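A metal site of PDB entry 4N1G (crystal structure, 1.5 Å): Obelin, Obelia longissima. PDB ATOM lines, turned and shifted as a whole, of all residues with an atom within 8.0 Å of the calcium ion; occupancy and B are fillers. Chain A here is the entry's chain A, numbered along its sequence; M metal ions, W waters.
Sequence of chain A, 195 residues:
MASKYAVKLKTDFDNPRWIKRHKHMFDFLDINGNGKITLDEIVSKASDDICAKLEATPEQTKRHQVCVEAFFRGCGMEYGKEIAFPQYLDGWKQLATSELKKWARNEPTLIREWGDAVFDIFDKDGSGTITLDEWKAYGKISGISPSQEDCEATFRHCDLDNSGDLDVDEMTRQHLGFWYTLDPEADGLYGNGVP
Of the 15 residues printed, 5 come within 4 Å of the calcium ion.
Water W1 lies within hydrogen-bond range of OE1 of Glu 82, ND2 of Asn 34 and ND2 of Asn 32.
The calcium ion is bound by the side-chain carboxylate (OD1) of Asp 30, water W1, the backbone carbonyl oxygen (O) of Lys 36, the side-chain amide oxygen (OD1) of Asn 32, the side-chain carboxylate (OE2) of Glu 41, the side-chain amide oxygen (OD1) of Asn 34 and the side-chain carboxylate (OE1) of Glu 41.
The backbone NH (N) of Ile 31 sits close to the side-chain carboxylate (OE2) of Glu 41, at 3.3 Å. The side-chain carboxylate (OD2) of Asp 30 is in hydrogen-bond range of the backbone NH (N) of Gly 35 (2.8 Å). The backbone NH (N) of Glu 41 lies within hydrogen-bond range of the side-chain hydroxyl (OG1) of Thr 38 (3.1 Å). OD1 of Asp 30 lies close to N of Gly 33 (3.2 Å). The side-chain amide nitrogen (ND2) of Asn 34 sits at hydrogen-bond distance from the side-chain carboxylate (OE1) of Glu 82 (3.2 Å).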
ATOM      1  N   PHE A  26     -10.679 -12.056  22.669  1.00  0.00           N
ATOM      2  CA  PHE A  26      -9.434 -11.820  21.924  1.00  0.00           C
ATOM      3  C   PHE A  26      -9.713 -11.292  20.526  1.00  0.00           C
ATOM      4  O   PHE A  26      -9.124 -10.282  20.103  1.00  0.00           O
ATOM      5  CB  PHE A  26      -8.616 -13.125  21.887  1.00  0.00           C
ATOM      6  CG  PHE A  26      -7.267 -12.983  21.161  1.00  0.00           C
ATOM      7  CD1 PHE A  26      -7.199 -13.155  19.822  1.00  0.00           C
ATOM      8  CD2 PHE A  26      -6.089 -12.721  21.873  1.00  0.00           C
ATOM      9  CE1 PHE A  26      -5.970 -13.103  19.143  1.00  0.00           C
ATOM     10  CE2 PHE A  26      -4.863 -12.645  21.211  1.00  0.00           C
ATOM     11  CZ  PHE A  26      -4.832 -12.808  19.827  1.00  0.00           C
ATOM     12  N   ASP A  27     -10.589 -11.946  19.779  1.00  0.00           N
ATOM     13  CA  ASP A  27     -10.896 -11.546  18.422  1.00  0.00           C
ATOM     14  C   ASP A  27     -11.536 -10.156  18.422  1.00  0.00           C
ATOM     15  O   ASP A  27     -11.240  -9.337  17.535  1.00  0.00           O
ATOM     16  CB  ASP A  27     -11.814 -12.569  17.771  1.00  0.00           C
ATOM     17  CG  ASP A  27     -11.104 -13.858  17.405  1.00  0.00           C
ATOM     18  OD1 ASP A  27      -9.835 -13.894  17.444  1.00  0.00           O
ATOM     19  OD2 ASP A  27     -11.840 -14.826  17.043  1.00  0.00           O
ATOM     20  N   LEU A  29     -11.049  -7.722  20.630  1.00  0.00           N
ATOM     21  CA  LEU A  29     -10.093  -6.713  21.106  1.00  0.00           C
ATOM     22  C   LEU A  29      -8.933  -6.540  20.090  1.00  0.00           C
ATOM     23  O   LEU A  29      -8.229  -5.494  20.152  1.00  0.00           O
ATOM     24  CB  LEU A  29      -9.540  -7.093  22.458  1.00  0.00           C
ATOM     25  CG  LEU A  29     -10.490  -7.162  23.663  1.00  0.00           C
ATOM     26  CD1 LEU A  29      -9.884  -7.855  24.868  1.00  0.00           C
ATOM     27  CD2 LEU A  29     -10.909  -5.772  24.113  1.00  0.00           C
ATOM     28  N   ASP A  30      -8.754  -7.484  19.181  1.00  0.00           N
ATOM     29  CA  ASP A  30      -7.720  -7.450  18.142  1.00  0.00           C
ATOM     30  C   ASP A  30      -8.159  -6.469  17.073  1.00  0.00           C
ATOM     31  O   ASP A  30      -8.583  -6.853  15.964  1.00  0.00           O
ATOM     32  CB  ASP A  30      -7.474  -8.843  17.602  1.00  0.00           C
ATOM     33  CG  ASP A  30      -6.406  -8.892  16.506  1.00  0.00           C
ATOM     34  OD1 ASP A  30      -5.641  -7.902  16.349  1.00  0.00           O
ATOM     35  OD2 ASP A  30      -6.379  -9.925  15.794  1.00  0.00           O
ATOM     36  N   ILE A  31      -8.082  -5.197  17.426  1.00  0.00           N
ATOM     37  CA  ILE A  31      -8.564  -4.097  16.581  1.00  0.00           C
ATOM     38  C   ILE A  31      -8.046  -4.197  15.134  1.00  0.00           C
ATOM     39  O   ILE A  31      -8.825  -4.073  14.161  1.00  0.00           O
ATOM     40  CB  ILE A  31      -8.146  -2.699  17.165  1.00  0.00           C
ATOM     41  CG1 ILE A  31      -8.709  -2.449  18.565  1.00  0.00           C
ATOM     42  CG2 ILE A  31      -8.516  -1.587  16.163  1.00  0.00           C
ATOM     43  CD1 ILE A  31      -8.236  -1.113  19.225  1.00  0.00           C
ATOM     44  N   ASN A  32      -6.737  -4.400  14.950  1.00  0.00           N
ATOM     45  CA  ASN A  32      -6.164  -4.405  13.590  1.00  0.00           C
ATOM     46  C   ASN A  32      -6.213  -5.772  12.938  1.00  0.00           C
ATOM     47  O   ASN A  32      -5.686  -5.996  11.842  1.00  0.00           O
ATOM     48  CB  ASN A  32      -4.715  -3.813  13.595  1.00  0.00           C
ATOM     49  CG  ASN A  32      -3.709  -4.635  14.380  1.00  0.00           C
ATOM     50  OD1 ASN A  32      -3.991  -5.766  14.780  1.00  0.00           O
ATOM     51  ND2 ASN A  32      -2.559  -4.037  14.677  1.00  0.00           N
ATOM     52  N   GLY A  33      -6.864  -6.719  13.621  1.00  0.00           N
ATOM     53  CA  GLY A  33      -7.107  -8.053  13.088  1.00  0.00           C
ATOM     54  C   GLY A  33      -5.886  -8.869  12.724  1.00  0.00           C
ATOM     55  O   GLY A  33      -5.985  -9.757  11.835  1.00  0.00           O
ATOM     56  N   ASN A  34      -4.734  -8.560  13.327  1.00  0.00           N
ATOM     57  CA  ASN A  34      -3.489  -9.241  12.919  1.00  0.00           C
ATOM     58  C   ASN A  34      -3.184 -10.541  13.706  1.00  0.00           C
ATOM     59  O   ASN A  34      -2.104 -11.154  13.534  1.00  0.00           O
ATOM     60  CB  ASN A  34      -2.319  -8.255  12.967  1.00  0.00           C
ATOM     61  CG  ASN A  34      -1.884  -7.884  14.358  1.00  0.00           C
ATOM     62  OD1 ASN A  34      -2.502  -8.243  15.333  1.00  0.00           O
ATOM     63  ND2 ASN A  34      -0.862  -7.068  14.451  1.00  0.00           N
ATOM     64  N   GLY A  35      -4.127 -10.982  14.542  1.00  0.00           N
ATOM     65  CA  GLY A  35      -3.967 -12.227  15.252  1.00  0.00           C
ATOM     66  C   GLY A  35      -3.071 -12.133  16.479  1.00  0.00           C
ATOM     67  O   GLY A  35      -2.732 -13.146  17.048  1.00  0.00           O
ATOM     68  N   LYS A  36      -2.706 -10.913  16.876  1.00  0.00           N
ATOM     69  CA  LYS A  36      -1.933 -10.647  18.071  1.00  0.00           C
ATOM     70  C   LYS A  36      -2.626  -9.570  18.830  1.00  0.00           C
ATOM     71  O   LYS A  36      -3.204  -8.647  18.226  1.00  0.00           O
ATOM     72  CB  LYS A  36      -0.507 -10.183  17.724  1.00  0.00           C
ATOM     73  CG  LYS A  36       0.242 -11.055  16.790  1.00  0.00           C
ATOM     74  CD  LYS A  36       0.748 -12.263  17.467  1.00  0.00           C
ATOM     75  CE  LYS A  36       2.011 -12.734  16.753  1.00  0.00           C
ATOM     76  NZ  LYS A  36       1.993 -12.257  15.348  1.00  0.00           N
ATOM     77  N   ILE A  37      -2.602  -9.625  20.158  1.00  0.00           N
ATOM     78  CA  ILE A  37      -3.233  -8.615  20.944  1.00  0.00           C
ATOM     79  C   ILE A  37      -2.135  -7.801  21.656  1.00  0.00           C
ATOM     80  O   ILE A  37      -1.059  -8.330  22.036  1.00  0.00           O
ATOM     81  CB  ILE A  37      -4.241  -9.241  21.966  1.00  0.00           C
ATOM     82  CG1 ILE A  37      -5.131  -8.172  22.542  1.00  0.00           C
ATOM     83  CG2 ILE A  37      -3.483  -9.936  23.089  1.00  0.00           C
ATOM     84  CD1 ILE A  37      -6.304  -8.770  23.255  1.00  0.00           C
ATOM     85  N   THR A  38      -2.388  -6.516  21.847  1.00  0.00           N
ATOM     86  CA  THR A  38      -1.460  -5.677  22.630  1.00  0.00           C
ATOM     87  C   THR A  38      -2.206  -4.970  23.749  1.00  0.00           C
ATOM     88  O   THR A  38      -3.450  -4.780  23.700  1.00  0.00           O
ATOM     89  CB  THR A  38      -0.790  -4.561  21.784  1.00  0.00           C
ATOM     90  OG1 THR A  38      -1.833  -3.661  21.286  1.00  0.00           O
ATOM     91  CG2 THR A  38      -0.015  -5.168  20.592  1.00  0.00           C
ATOM     92  N   GLU A  41      -4.302  -2.134  22.298  1.00  0.00           N
ATOM     93  CA  GLU A  41      -5.641  -2.553  21.801  1.00  0.00           C
ATOM     94  C   GLU A  41      -6.624  -2.798  22.962  1.00  0.00           C
ATOM     95  O   GLU A  41      -7.815  -2.305  22.922  1.00  0.00           O
ATOM     96  CB  GLU A  41      -5.490  -3.797  20.962  1.00  0.00           C
ATOM     97  CG  GLU A  41      -4.877  -3.523  19.579  1.00  0.00           C
ATOM     98  CD  GLU A  41      -4.696  -4.767  18.727  1.00  0.00           C
ATOM     99  OE1 GLU A  41      -4.412  -5.888  19.262  1.00  0.00           O
ATOM    100  OE2 GLU A  41      -4.801  -4.659  17.459  1.00  0.00           O
ATOM    101  N   GLU A  82       3.294  -7.630  21.218  1.00  0.00           N
ATOM    102  CA  GLU A  82       2.233  -8.355  20.477  1.00  0.00           C
ATOM    103  C   GLU A  82       2.150  -9.773  20.951  1.00  0.00           C
ATOM    104  O   GLU A  82       3.136 -10.521  20.813  1.00  0.00           O
ATOM    105  CB  GLU A  82       2.523  -8.339  19.013  1.00  0.00           C
ATOM    106  CG  GLU A  82       2.834  -6.932  18.525  1.00  0.00           C
ATOM    107  CD  GLU A  82       1.744  -6.271  17.736  1.00  0.00           C
ATOM    108  OE1 GLU A  82       0.855  -6.963  17.188  1.00  0.00           O
ATOM    109  OE2 GLU A  82       1.823  -5.000  17.637  1.00  0.00           O
ATOM    110  N   ILE A  83       0.980 -10.193  21.406  1.00  0.00           N
ATOM    111  CA  ILE A  83       0.877 -11.556  21.985  1.00  0.00           C
ATOM    112  C   ILE A  83      -0.204 -12.372  21.288  1.00  0.00           C
ATOM    113  O   ILE A  83      -1.340 -11.877  21.120  1.00  0.00           O
ATOM    114  CB  ILE A  83       0.602 -11.457  23.503  1.00  0.00           C
ATOM    115  CG1 ILE A  83       1.857 -10.851  24.145  1.00  0.00           C
ATOM    116  CG2 ILE A  83       0.295 -12.861  24.119  1.00  0.00           C
ATOM    117  CD1 ILE A  83       1.687 -10.445  25.501  1.00  0.00           C
HETATM  118 CA    CA M   1      -3.720  -6.775  16.938  1.00  0.00          CA
HETATM  119  O   HOH W   1      -1.670  -5.774  17.300  1.00  0.00           O
